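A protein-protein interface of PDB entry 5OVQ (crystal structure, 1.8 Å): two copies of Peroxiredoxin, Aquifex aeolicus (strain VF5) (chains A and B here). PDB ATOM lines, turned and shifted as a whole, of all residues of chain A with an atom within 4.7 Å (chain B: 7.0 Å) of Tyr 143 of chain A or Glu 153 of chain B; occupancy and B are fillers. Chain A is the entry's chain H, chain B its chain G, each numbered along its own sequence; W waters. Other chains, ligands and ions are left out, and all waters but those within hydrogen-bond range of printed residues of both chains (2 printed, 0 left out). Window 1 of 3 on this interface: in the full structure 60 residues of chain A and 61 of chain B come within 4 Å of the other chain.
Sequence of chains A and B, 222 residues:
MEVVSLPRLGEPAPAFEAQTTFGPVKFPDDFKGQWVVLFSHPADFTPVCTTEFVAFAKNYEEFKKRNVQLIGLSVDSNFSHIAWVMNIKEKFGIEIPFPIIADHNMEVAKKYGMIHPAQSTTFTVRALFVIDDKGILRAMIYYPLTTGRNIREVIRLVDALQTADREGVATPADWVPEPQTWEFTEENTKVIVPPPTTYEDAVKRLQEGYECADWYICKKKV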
ATOM      1  N   VAL A 125      11.300 -34.901   3.992  1.00  0.00           N
ATOM      2  CA  VAL A 125      11.745 -33.960   5.014  1.00  0.00           C
ATOM      3  C   VAL A 125      12.333 -32.749   4.304  1.00  0.00           C
ATOM      4  O   VAL A 125      12.275 -32.651   3.072  1.00  0.00           O
ATOM      5  CB  VAL A 125      12.758 -34.628   5.963  1.00  0.00           C
ATOM      6  CG1 VAL A 125      12.115 -35.851   6.617  1.00  0.00           C
ATOM      7  CG2 VAL A 125      14.040 -35.001   5.217  1.00  0.00           C
ATOM      8  N   ARG A 126      12.935 -31.835   5.060  1.00  0.00           N
ATOM      9  CA  ARG A 126      13.546 -30.640   4.477  1.00  0.00           C
ATOM     10  C   ARG A 126      15.012 -30.934   4.162  1.00  0.00           C
ATOM     11  O   ARG A 126      15.934 -30.494   4.848  1.00  0.00           O
ATOM     12  CB  ARG A 126      13.419 -29.461   5.428  1.00  0.00           C
ATOM     13  CG  ARG A 126      12.015 -29.206   5.873  1.00  0.00           C
ATOM     14  CD  ARG A 126      11.899 -27.924   6.720  1.00  0.00           C
ATOM     15  NE  ARG A 126      10.514 -27.858   7.141  1.00  0.00           N
ATOM     16  CZ  ARG A 126       9.546 -27.430   6.345  1.00  0.00           C
ATOM     17  NH1 ARG A 126       9.862 -26.964   5.142  1.00  0.00           N
ATOM     18  NH2 ARG A 126       8.281 -27.449   6.755  1.00  0.00           N
ATOM     19  N   ILE A 141      22.068 -31.337   3.940  1.00  0.00           N
ATOM     20  CA  ILE A 141      21.365 -30.925   5.143  1.00  0.00           C
ATOM     21  C   ILE A 141      20.063 -31.704   5.200  1.00  0.00           C
ATOM     22  O   ILE A 141      19.415 -31.895   4.168  1.00  0.00           O
ATOM     23  CB  ILE A 141      21.039 -29.416   5.072  1.00  0.00           C
ATOM     24  CG1 ILE A 141      22.299 -28.572   4.885  1.00  0.00           C
ATOM     25  CG2 ILE A 141      20.165 -28.971   6.231  1.00  0.00           C
ATOM     26  CD1 ILE A 141      23.277 -28.740   5.946  1.00  0.00           C
ATOM     27  N   TYR A 142      19.661 -32.133   6.396  1.00  0.00           N
ATOM     28  CA  TYR A 142      18.347 -32.747   6.595  1.00  0.00           C
ATOM     29  C   TYR A 142      17.690 -32.085   7.802  1.00  0.00           C
ATOM     30  O   TYR A 142      17.982 -32.432   8.951  1.00  0.00           O
ATOM     31  CB  TYR A 142      18.408 -34.261   6.795  1.00  0.00           C
ATOM     32  CG  TYR A 142      18.886 -35.092   5.626  1.00  0.00           C
ATOM     33  CD1 TYR A 142      17.983 -35.651   4.746  1.00  0.00           C
ATOM     34  CD2 TYR A 142      20.243 -35.266   5.375  1.00  0.00           C
ATOM     35  CE1 TYR A 142      18.408 -36.417   3.666  1.00  0.00           C
ATOM     36  CE2 TYR A 142      20.678 -36.029   4.309  1.00  0.00           C
ATOM     37  CZ  TYR A 142      19.763 -36.602   3.455  1.00  0.00           C
ATOM     38  OH  TYR A 142      20.199 -37.358   2.386  1.00  0.00           O
ATOM     39  N   TYR A 143      16.774 -31.180   7.544  1.00  0.00           N
ATOM     40  CA  TYR A 143      16.035 -30.575   8.637  1.00  0.00           C
ATOM     41  C   TYR A 143      14.656 -31.212   8.757  1.00  0.00           C
ATOM     42  O   TYR A 143      14.129 -31.747   7.779  1.00  0.00           O
ATOM     43  CB  TYR A 143      15.896 -29.064   8.425  1.00  0.00           C
ATOM     44  CG  TYR A 143      17.093 -28.241   8.885  1.00  0.00           C
ATOM     45  CD1 TYR A 143      18.340 -28.830   9.112  1.00  0.00           C
ATOM     46  CD2 TYR A 143      16.967 -26.873   9.095  1.00  0.00           C
ATOM     47  CE1 TYR A 143      19.423 -28.060   9.528  1.00  0.00           C
ATOM     48  CE2 TYR A 143      18.036 -26.107   9.513  1.00  0.00           C
ATOM     49  CZ  TYR A 143      19.262 -26.700   9.729  1.00  0.00           C
ATOM     50  OH  TYR A 143      20.335 -25.931  10.150  1.00  0.00           O
ATOM     51  N   PRO A 144      14.043 -31.195   9.933  1.00  0.00           N
ATOM     52  CA  PRO A 144      12.745 -31.850  10.105  1.00  0.00           C
ATOM     53  C   PRO A 144      11.603 -30.980   9.589  1.00  0.00           C
ATOM     54  O   PRO A 144      11.789 -29.838   9.182  1.00  0.00           O
ATOM     55  CB  PRO A 144      12.650 -32.038  11.615  1.00  0.00           C
ATOM     56  CG  PRO A 144      13.426 -30.899  12.161  1.00  0.00           C
ATOM     57  CD  PRO A 144      14.597 -30.731  11.221  1.00  0.00           C
ATOM     58  N   LEU A 145      10.398 -31.556   9.622  1.00  0.00           N
ATOM     59  CA  LEU A 145       9.224 -30.877   9.086  1.00  0.00           C
ATOM     60  C   LEU A 145       8.935 -29.571   9.813  1.00  0.00           C
ATOM     61  O   LEU A 145       8.383 -28.647   9.218  1.00  0.00           O
ATOM     62  CB  LEU A 145       8.003 -31.792   9.157  1.00  0.00           C
ATOM     63  CG  LEU A 145       8.131 -33.132   8.440  1.00  0.00           C
ATOM     64  CD1 LEU A 145       6.842 -33.924   8.584  1.00  0.00           C
ATOM     65  CD2 LEU A 145       8.482 -32.914   6.973  1.00  0.00           C
ATOM     66  N   THR A 147      10.942 -27.224  10.913  1.00  0.00           N
ATOM     67  CA  THR A 147      12.015 -26.247  11.090  1.00  0.00           C
ATOM     68  C   THR A 147      12.521 -25.713   9.758  1.00  0.00           C
ATOM     69  O   THR A 147      13.231 -26.416   9.032  1.00  0.00           O
ATOM     70  CB  THR A 147      13.153 -26.883  11.891  1.00  0.00           C
ATOM     71  OG1 THR A 147      12.601 -27.390  13.112  1.00  0.00           O
ATOM     72  CG2 THR A 147      14.228 -25.857  12.208  1.00  0.00           C
ATOM     73  N   GLY A 148      12.178 -24.462   9.450  1.00  0.00           N
ATOM     74  CA  GLY A 148      12.657 -23.859   8.220  1.00  0.00           C
ATOM     75  C   GLY A 148      14.165 -23.696   8.204  1.00  0.00           C
ATOM     76  O   GLY A 148      14.810 -23.508   9.237  1.00  0.00           O
ATOM     77  N   ARG A 149      14.718 -23.723   6.993  1.00  0.00           N
ATOM     78  CA  ARG A 149      16.147 -23.671   6.754  1.00  0.00           C
ATOM     79  C   ARG A 149      16.652 -22.224   6.776  1.00  0.00           C
ATOM     80  O   ARG A 149      15.881 -21.265   6.802  1.00  0.00           O
ATOM     81  CB  ARG A 149      16.456 -24.367   5.427  1.00  0.00           C
ATOM     82  CG  ARG A 149      16.331 -25.901   5.541  1.00  0.00           C
ATOM     83  CD  ARG A 149      16.122 -26.618   4.192  1.00  0.00           C
ATOM     84  NE  ARG A 149      14.738 -26.474   3.738  1.00  0.00           N
ATOM     85  CZ  ARG A 149      14.144 -27.288   2.870  1.00  0.00           C
ATOM     86  NH1 ARG A 149      14.805 -28.314   2.352  1.00  0.00           N
ATOM     87  NH2 ARG A 149      12.883 -27.076   2.530  1.00  0.00           N
ATOM     88  N   ASN A 150      17.974 -22.081   6.766  1.00  0.00           N
ATOM     89  CA  ASN A 150      18.650 -20.788   6.844  1.00  0.00           C
ATOM     90  C   ASN A 150      19.190 -20.520   5.443  1.00  0.00           C
ATOM     91  O   ASN A 150      20.173 -21.130   5.023  1.00  0.00           O
ATOM     92  CB  ASN A 150      19.754 -20.834   7.903  1.00  0.00           C
ATOM     93  CG  ASN A 150      20.421 -19.503   8.109  1.00  0.00           C
ATOM     94  OD1 ASN A 150      20.462 -18.669   7.207  1.00  0.00           O
ATOM     95  ND2 ASN A 150      20.951 -19.290   9.312  1.00  0.00           N
ATOM     96  N   GLU A 153      22.781 -19.376   5.087  1.00  0.00           N
ATOM     97  CA  GLU A 153      23.782 -20.430   5.287  1.00  0.00           C
ATOM     98  C   GLU A 153      23.956 -21.268   4.025  1.00  0.00           C
ATOM     99  O   GLU A 153      25.062 -21.737   3.733  1.00  0.00           O
ATOM    100  CB  GLU A 153      23.408 -21.313   6.480  1.00  0.00           C
ATOM    101  CG  GLU A 153      24.315 -22.564   6.692  1.00  0.00           C
ATOM    102  CD  GLU A 153      25.808 -22.234   6.900  1.00  0.00           C
ATOM    103  OE1 GLU A 153      26.158 -21.065   7.183  1.00  0.00           O
ATOM    104  OE2 GLU A 153      26.636 -23.167   6.781  1.00  0.00           O
ATOM    105  N   LEU B   9      15.568 -39.520  10.912  1.00  0.00           N
ATOM    106  CA  LEU B   9      14.990 -38.451  11.709  1.00  0.00           C
ATOM    107  C   LEU B   9      13.725 -38.926  12.404  1.00  0.00           C
ATOM    108  O   LEU B   9      12.897 -39.631  11.819  1.00  0.00           O
ATOM    109  CB  LEU B   9      14.669 -37.242  10.832  1.00  0.00           C
ATOM    110  CG  LEU B   9      15.846 -36.544  10.156  1.00  0.00           C
ATOM    111  CD1 LEU B   9      15.347 -35.347   9.371  1.00  0.00           C
ATOM    112  CD2 LEU B   9      16.898 -36.110  11.191  1.00  0.00           C
ATOM    113  N   ARG B 138      16.814 -35.373  15.714  1.00  0.00           N
ATOM    114  CA  ARG B 138      15.915 -34.315  15.270  1.00  0.00           C
ATOM    115  C   ARG B 138      16.321 -33.651  13.962  1.00  0.00           C
ATOM    116  O   ARG B 138      15.449 -33.181  13.231  1.00  0.00           O
ATOM    117  CB  ARG B 138      15.803 -33.224  16.350  1.00  0.00           C
ATOM    118  CG  ARG B 138      15.330 -33.752  17.699  1.00  0.00           C
ATOM    119  CD  ARG B 138      13.913 -34.311  17.591  1.00  0.00           C
ATOM    120  NE  ARG B 138      12.976 -33.248  17.245  1.00  0.00           N
ATOM    121  CZ  ARG B 138      12.312 -32.516  18.134  1.00  0.00           C
ATOM    122  NH1 ARG B 138      12.456 -32.746  19.434  1.00  0.00           N
ATOM    123  NH2 ARG B 138      11.499 -31.555  17.722  1.00  0.00           N
ATOM    124  N   ALA B 139      17.610 -33.578  13.658  1.00  0.00           N
ATOM    125  CA  ALA B 139      18.101 -32.869  12.485  1.00  0.00           C
ATOM    126  C   ALA B 139      19.552 -33.267  12.285  1.00  0.00           C
ATOM    127  O   ALA B 139      20.233 -33.681  13.228  1.00  0.00           O
ATOM    128  CB  ALA B 139      17.981 -31.338  12.637  1.00  0.00           C
ATOM    129  N   MET B 140      20.029 -33.127  11.053  1.00  0.00           N
ATOM    130  CA  MET B 140      21.423 -33.479  10.836  1.00  0.00           C
ATOM    131  C   MET B 140      21.967 -32.743   9.626  1.00  0.00           C
ATOM    132  O   MET B 140      21.215 -32.324   8.737  1.00  0.00           O
ATOM    133  CB  MET B 140      21.584 -34.986  10.663  1.00  0.00           C
ATOM    134  CG  MET B 140      20.985 -35.553   9.386  1.00  0.00           C
ATOM    135  SD  MET B 140      20.861 -37.350   9.551  1.00  0.00           S
ATOM    136  CE  MET B 140      19.207 -37.585   8.918  1.00  0.00           C
ATOM    137  N   ILE B 141      23.284 -32.555   9.626  1.00  0.00           N
ATOM    138  CA  ILE B 141      23.983 -31.929   8.516  1.00  0.00           C
ATOM    139  C   ILE B 141      25.257 -32.717   8.253  1.00  0.00           C
ATOM    140  O   ILE B 141      25.865 -33.279   9.169  1.00  0.00           O
ATOM    141  CB  ILE B 141      24.288 -30.435   8.766  1.00  0.00           C
ATOM    142  CG1 ILE B 141      25.514 -30.250   9.636  1.00  0.00           C
ATOM    143  CG2 ILE B 141      23.057 -29.690   9.352  1.00  0.00           C
ATOM    144  CD1 ILE B 141      26.136 -28.887   9.483  1.00  0.00           C
ATOM    145  N   TYR B 143      28.712 -31.754   6.267  1.00  0.00           N
ATOM    146  CA  TYR B 143      29.575 -30.900   5.468  1.00  0.00           C
ATOM    147  C   TYR B 143      30.840 -31.656   5.075  1.00  0.00           C
ATOM    148  O   TYR B 143      31.249 -32.602   5.759  1.00  0.00           O
ATOM    149  CB  TYR B 143      29.954 -29.622   6.231  1.00  0.00           C
ATOM    150  CG  TYR B 143      28.890 -28.522   6.165  1.00  0.00           C
ATOM    151  CD1 TYR B 143      27.571 -28.807   5.803  1.00  0.00           C
ATOM    152  CD2 TYR B 143      29.211 -27.208   6.454  1.00  0.00           C
ATOM    153  CE1 TYR B 143      26.598 -27.795   5.750  1.00  0.00           C
ATOM    154  CE2 TYR B 143      28.248 -26.197   6.405  1.00  0.00           C
ATOM    155  CZ  TYR B 143      26.948 -26.493   6.055  1.00  0.00           C
ATOM    156  OH  TYR B 143      26.006 -25.465   6.010  1.00  0.00           O
ATOM    157  N   ARG B 149      31.800 -25.580   9.608  1.00  0.00           N
ATOM    158  CA  ARG B 149      30.387 -25.404   9.884  1.00  0.00           C
ATOM    159  C   ARG B 149      30.096 -24.008  10.451  1.00  0.00           C
ATOM    160  O   ARG B 149      30.999 -23.236  10.809  1.00  0.00           O
ATOM    161  CB  ARG B 149      29.930 -26.505  10.833  1.00  0.00           C
ATOM    162  CG  ARG B 149      29.856 -27.864  10.138  1.00  0.00           C
ATOM    163  CD  ARG B 149      29.907 -29.047  11.095  1.00  0.00           C
ATOM    164  NE  ARG B 149      31.277 -29.345  11.538  1.00  0.00           N
ATOM    165  CZ  ARG B 149      31.662 -30.534  11.999  1.00  0.00           C
ATOM    166  NH1 ARG B 149      30.794 -31.525  12.071  1.00  0.00           N
ATOM    167  NH2 ARG B 149      32.915 -30.734  12.391  1.00  0.00           N
ATOM    168  N   ASN B 150      28.799 -23.698  10.558  1.00  0.00           N
ATOM    169  CA  ASN B 150      28.300 -22.410  11.039  1.00  0.00           C
ATOM    170  C   ASN B 150      27.755 -22.645  12.444  1.00  0.00           C
ATOM    171  O   ASN B 150      26.705 -23.268  12.609  1.00  0.00           O
ATOM    172  CB  ASN B 150      27.230 -21.871  10.085  1.00  0.00           C
ATOM    173  CG  ASN B 150      26.697 -20.509  10.490  1.00  0.00           C
ATOM    174  OD1 ASN B 150      26.672 -20.157  11.667  1.00  0.00           O
ATOM    175  ND2 ASN B 150      26.261 -19.728   9.497  1.00  0.00           N
ATOM    176  N   ILE B 151      28.500 -22.203  13.462  1.00  0.00           N
ATOM    177  CA  ILE B 151      28.138 -22.564  14.832  1.00  0.00           C
ATOM    178  C   ILE B 151      26.853 -21.849  15.254  1.00  0.00           C
ATOM    179  O   ILE B 151      26.016 -22.415  15.970  1.00  0.00           O
ATOM    180  CB  ILE B 151      29.306 -22.281  15.803  1.00  0.00           C
ATOM    181  CG1 ILE B 151      30.312 -23.440  15.821  1.00  0.00           C
ATOM    182  CG2 ILE B 151      28.791 -22.105  17.215  1.00  0.00           C
ATOM    183  CD1 ILE B 151      31.067 -23.665  14.520  1.00  0.00           C
ATOM    184  N   ARG B 152      26.664 -20.605  14.813  1.00  0.00           N
ATOM    185  CA  ARG B 152      25.432 -19.901  15.171  1.00  0.00           C
ATOM    186  C   ARG B 152      24.204 -20.548  14.540  1.00  0.00           C
ATOM    187  O   ARG B 152      23.119 -20.502  15.127  1.00  0.00           O
ATOM    188  CB  ARG B 152      25.525 -18.422  14.798  1.00  0.00           C
ATOM    189  CG  ARG B 152      26.333 -17.626  15.844  1.00  0.00           C
ATOM    190  CD  ARG B 152      26.527 -16.185  15.440  1.00  0.00           C
ATOM    191  NE  ARG B 152      27.401 -16.082  14.278  1.00  0.00           N
ATOM    192  CZ  ARG B 152      28.108 -15.003  13.959  1.00  0.00           C
ATOM    193  NH1 ARG B 152      28.069 -13.917  14.726  1.00  0.00           N
ATOM    194  NH2 ARG B 152      28.865 -15.020  12.869  1.00  0.00           N
ATOM    195  N   GLU B 153      24.349 -21.170  13.368  1.00  0.00           N
ATOM    196  CA  GLU B 153      23.218 -21.904  12.794  1.00  0.00           C
ATOM    197  C   GLU B 153      22.884 -23.148  13.607  1.00  0.00           C
ATOM    198  O   GLU B 153      21.713 -23.540  13.684  1.00  0.00           O
ATOM    199  CB  GLU B 153      23.505 -22.286  11.338  1.00  0.00           C
ATOM    200  CG  GLU B 153      22.444 -23.208  10.675  1.00  0.00           C
ATOM    201  CD  GLU B 153      21.024 -22.628  10.660  1.00  0.00           C
ATOM    202  OE1 GLU B 153      20.844 -21.409  10.873  1.00  0.00           O
ATOM    203  OE2 GLU B 153      20.072 -23.410  10.427  1.00  0.00           O
ATOM    204  N   VAL B 154      23.893 -23.783  14.220  1.00  0.00           N
ATOM    205  CA  VAL B 154      23.612 -24.894  15.122  1.00  0.00           C
ATOM    206  C   VAL B 154      22.783 -24.406  16.300  1.00  0.00           C
ATOM    207  O   VAL B 154      21.807 -25.048  16.705  1.00  0.00           O
ATOM    208  CB  VAL B 154      24.924 -25.545  15.603  1.00  0.00           C
ATOM    209  CG1 VAL B 154      24.602 -26.698  16.532  1.00  0.00           C
ATOM    210  CG2 VAL B 154      25.758 -25.987  14.422  1.00  0.00           C
ATOM    211  N   ILE B 155      23.154 -23.254  16.861  1.00  0.00           N
ATOM    212  CA  ILE B 155      22.393 -22.696  17.975  1.00  0.00           C
ATOM    213  C   ILE B 155      20.983 -22.323  17.531  1.00  0.00           C
ATOM    214  O   ILE B 155      20.002 -22.617  18.225  1.00  0.00           O
ATOM    215  CB  ILE B 155      23.144 -21.491  18.568  1.00  0.00           C
ATOM    216  CG1 ILE B 155      24.472 -21.962  19.156  1.00  0.00           C
ATOM    217  CG2 ILE B 155      22.300 -20.785  19.606  1.00  0.00           C
ATOM    218  CD1 ILE B 155      25.390 -20.852  19.568  1.00  0.00           C
ATOM    219  N   ARG B 156      20.853 -21.684  16.363  1.00  0.00           N
ATOM    220  CA  ARG B 156      19.529 -21.311  15.862  1.00  0.00           C
ATOM    221  C   ARG B 156      18.670 -22.546  15.640  1.00  0.00           C
ATOM    222  O   ARG B 156      17.467 -22.546  15.937  1.00  0.00           O
ATOM    223  CB  ARG B 156      19.660 -20.530  14.557  1.00  0.00           C
ATOM    224  CG  ARG B 156      18.345 -19.893  14.060  1.00  0.00           C
ATOM    225  CD  ARG B 156      18.467 -19.522  12.605  1.00  0.00           C
ATOM    226  NE  ARG B 156      18.434 -20.707  11.759  1.00  0.00           N
ATOM    227  CZ  ARG B 156      17.329 -21.302  11.319  1.00  0.00           C
ATOM    228  NH1 ARG B 156      16.124 -20.826  11.623  1.00  0.00           N
ATOM    229  NH2 ARG B 156      17.430 -22.392  10.566  1.00  0.00           N
ATOM    230  N   LEU B 157      19.279 -23.605  15.106  1.00  0.00           N
ATOM    231  CA  LEU B 157      18.570 -24.861  14.898  1.00  0.00           C
ATOM    232  C   LEU B 157      18.064 -25.434  16.216  1.00  0.00           C
ATOM    233  O   LEU B 157      16.909 -25.865  16.312  1.00  0.00           O
ATOM    234  CB  LEU B 157      19.492 -25.849  14.198  1.00  0.00           C
ATOM    235  CG  LEU B 157      18.977 -27.261  13.970  1.00  0.00           C
ATOM    236  CD1 LEU B 157      17.667 -27.255  13.155  1.00  0.00           C
ATOM    237  CD2 LEU B 157      20.057 -28.085  13.297  1.00  0.00           C
ATOM    238  N   VAL B 158      18.913 -25.432  17.248  1.00  0.00           N
ATOM    239  CA  VAL B 158      18.490 -25.900  18.566  1.00  0.00           C
ATOM    240  C   VAL B 158      17.334 -25.053  19.088  1.00  0.00           C
ATOM    241  O   VAL B 158      16.361 -25.575  19.641  1.00  0.00           O
ATOM    242  CB  VAL B 158      19.675 -25.891  19.547  1.00  0.00           C
ATOM    243  CG1 VAL B 158      19.180 -26.148  20.964  1.00  0.00           C
ATOM    244  CG2 VAL B 158      20.743 -26.903  19.119  1.00  0.00           C
ATOM    245  N   ASP B 159      17.464 -23.727  18.988  1.00  0.00           N
ATOM    246  CA  ASP B 159      16.386 -22.831  19.400  1.00  0.00           C
ATOM    247  C   ASP B 159      15.091 -23.134  18.653  1.00  0.00           C
ATOM    248  O   ASP B 159      14.006 -23.140  19.248  1.00  0.00           O
ATOM    249  CB  ASP B 159      16.793 -21.373  19.178  1.00  0.00           C
ATOM    250  CG  ASP B 159      17.679 -20.833  20.272  1.00  0.00           C
ATOM    251  OD1 ASP B 159      17.641 -21.358  21.410  1.00  0.00           O
ATOM    252  OD2 ASP B 159      18.389 -19.843  19.996  1.00  0.00           O
ATOM    253  N   LEU B 161      14.153 -25.980  17.206  1.00  0.00           N
ATOM    254  CA  LEU B 161      13.593 -27.267  17.605  1.00  0.00           C
ATOM    255  C   LEU B 161      12.994 -27.196  19.000  1.00  0.00           C
ATOM    256  O   LEU B 161      11.938 -27.784  19.262  1.00  0.00           O
ATOM    257  CB  LEU B 161      14.670 -28.354  17.539  1.00  0.00           C
ATOM    258  CG  LEU B 161      15.139 -28.719  16.131  1.00  0.00           C
ATOM    259  CD1 LEU B 161      16.469 -29.415  16.200  1.00  0.00           C
ATOM    260  CD2 LEU B 161      14.102 -29.616  15.448  1.00  0.00           C
ATOM    261  N   ASP B 174      14.682 -18.859   8.192  1.00  0.00           N
ATOM    262  CA  ASP B 174      15.440 -17.767   8.807  1.00  0.00           C
ATOM    263  C   ASP B 174      14.866 -17.326  10.155  1.00  0.00           C
ATOM    264  O   ASP B 174      15.115 -16.191  10.596  1.00  0.00           O
ATOM    265  CB  ASP B 174      15.512 -16.554   7.867  1.00  0.00           C
ATOM    266  CG  ASP B 174      16.020 -16.910   6.484  1.00  0.00           C
ATOM    267  OD1 ASP B 174      17.010 -17.659   6.374  1.00  0.00           O
ATOM    268  OD2 ASP B 174      15.401 -16.462   5.497  1.00  0.00           O
ATOM    269  N   TRP B 175      14.132 -18.200  10.840  1.00  0.00           N
ATOM    270  CA  TRP B 175      13.539 -17.849  12.125  1.00  0.00           C
ATOM    271  C   TRP B 175      14.595 -17.707  13.215  1.00  0.00           C
ATOM    272  O   TRP B 175      15.525 -18.508  13.306  1.00  0.00           O
ATOM    273  CB  TRP B 175      12.533 -18.913  12.560  1.00  0.00           C
ATOM    274  CG  TRP B 175      11.958 -18.645  13.930  1.00  0.00           C
ATOM    275  CD1 TRP B 175      10.886 -17.857  14.227  1.00  0.00           C
ATOM    276  CD2 TRP B 175      12.456 -19.137  15.187  1.00  0.00           C
ATOM    277  NE1 TRP B 175      10.668 -17.844  15.586  1.00  0.00           N
ATOM    278  CE2 TRP B 175      11.617 -18.622  16.196  1.00  0.00           C
ATOM    279  CE3 TRP B 175      13.521 -19.967  15.553  1.00  0.00           C
ATOM    280  CZ2 TRP B 175      11.812 -18.907  17.548  1.00  0.00           C
ATOM    281  CZ3 TRP B 175      13.715 -20.248  16.897  1.00  0.00           C
ATOM    282  CH2 TRP B 175      12.860 -19.726  17.875  1.00  0.00           C
ATOM    283  N   TRP B 182      23.961 -11.387  13.184  1.00  0.00           N
ATOM    284  CA  TRP B 182      25.146 -12.241  13.165  1.00  0.00           C
ATOM    285  C   TRP B 182      26.244 -11.492  12.430  1.00  0.00           C
ATOM    286  O   TRP B 182      26.194 -11.350  11.204  1.00  0.00           O
ATOM    287  CB  TRP B 182      24.888 -13.592  12.497  1.00  0.00           C
ATOM    288  CG  TRP B 182      23.845 -14.395  13.147  1.00  0.00           C
ATOM    289  CD1 TRP B 182      23.056 -14.033  14.206  1.00  0.00           C
ATOM    290  CD2 TRP B 182      23.454 -15.720  12.783  1.00  0.00           C
ATOM    291  NE1 TRP B 182      22.181 -15.057  14.510  1.00  0.00           N
ATOM    292  CE2 TRP B 182      22.414 -16.104  13.655  1.00  0.00           C
ATOM    293  CE3 TRP B 182      23.886 -16.624  11.805  1.00  0.00           C
ATOM    294  CZ2 TRP B 182      21.801 -17.347  13.577  1.00  0.00           C
ATOM    295  CZ3 TRP B 182      23.270 -17.850  11.721  1.00  0.00           C
ATOM    296  CH2 TRP B 182      22.234 -18.206  12.600  1.00  0.00           C
HETATM  297  O   HOH W   1      13.309 -22.299  11.354  1.00  0.00           O
HETATM  298  O   HOH W   2      19.283 -16.429   6.926  1.00  0.00           O
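The backbone carbonyl oxygen (O) of Met 140 of chain B is in hydrogen-bond range of the backbone NH (N) of Tyr 142 of chain A, at 2.8 Å.
OE2 of Glu 153 of chain A lies within hydrogen-bond range of OH of Tyr 143 of chain B (2.5 Å).
ND2 of Asn 150 of chain B is in hydrogen-bond range of OE1 of Glu 153 of chain A, at 2.7 Å.
OH of Tyr 143 of chain A sits at hydrogen-bond distance from OE2 of Glu 153 of chain B (2.5 Å).
The side-chain carboxylate of Glu 153 of chain B is in hydrogen-bond range of the side-chain amide nitrogen of Asn 150 of chain A (2.6 Å).
NH2 of Arg 156 of chain B lies within hydrogen-bond range of O of Gly 148 of chain A (3.1 Å).
The backbone NH (N) of Asp 174 of chain B is in hydrogen-bond range of the backbone carbonyl oxygen (O) of Arg 149 of chain A, at 3.0 Å.
The backbone carbonyl oxygen (O) of Pro 144 of chain A is in hydrogen-bond range of the guanidinium group (NE) of Arg 126 of chain A (3.1 Å).
The side-chain amide oxygen of Asn 150 of chain A lies within hydrogen-bond range of the backbone NH of Glu 153 of chain A.
Among the printed residues, pairs that only touch across the chains: Ile 141 of chain A with Met 140 of chain B, Ile 141 of chain A with Ile 141 of chain B, Ile 141 of chain A with Tyr 143 of chain B, Tyr 142 of chain A with Leu 9 of chain B, Tyr 142 of chain A with Ala 139 of chain B, Tyr 143 of chain A with Ile 141 of chain B, Tyr 143 of chain A with Arg 156 of chain B, Tyr 143 of chain A with Leu 157 of chain B, Pro 144 of chain A with Arg 138 of chain B, Pro 144 of chain A with Ala 139 of chain B, Pro 144 of chain A with Leu 161 of chain B, Thr 147 of chain A with Leu 157 of chain B, Thr 147 of chain A with Leu 161 of chain B, Arg 149 of chain A with Arg 156 of chain B, Asn 150 of chain A with Arg 156 of chain B, Asn 150 of chain A with Asp 174 of chain B and Asn 150 of chain A with Trp 182 of chain B.
Of the printed residues of chain B, Tyr 143 of chain A touches Ile 141, Glu 153, Arg 156 and Leu 157.
Printed residues of chain A within 4 Å of Met 140 of chain B: Ile 141 and Tyr 142.
Printed residues of chain A within 4 Å of Trp 182 of chain B: Asn 150 (3.6 Å).
Val 125 of chain A touches none of the printed residues of chain B.
Val 154 of chain B touches none of the printed residues of chain A.
The nearest residue of chain A that does not touch Glu 153 of chain B is Glu 153 of chain A (4.4 Å).
The nearest printed residue of chain B that does not touch Asn 150 of chain A is Asn 150 of chain B (5.3 Å).
Hydrophobic or aromatic side chains of chain A that line the printed part of chain B: Ile 141, Tyr 142, Tyr 143 and Pro 144.
Among the printed residues, no Asp or Glu carboxylate lies within 4 Å of a Lys or Arg side-chain nitrogen of the other chain.
Ile 141 of chain A touches its own counterpart, Ile 141 of chain B.
Ile 141 of chain A touches Tyr 143 of chain B, and with the chains exchanged Tyr 143 of chain A touches Ile 141 of chain B.
Asn 150 of chain A touches Glu 153 of chain B, and with the chains exchanged Glu 153 of chain A touches Asn 150 of chain B.
Water W2 bridges OD1 of Asn 150 of chain A (2.5 Å) and OD1 of Asp 174 of chain B (2.6 Å).
Water W1 bridges the backbone carbonyl oxygen of Gly 148 of chain A (2.9 Å) and the guanidinium group of Arg 156 of chain B (3.2 Å).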
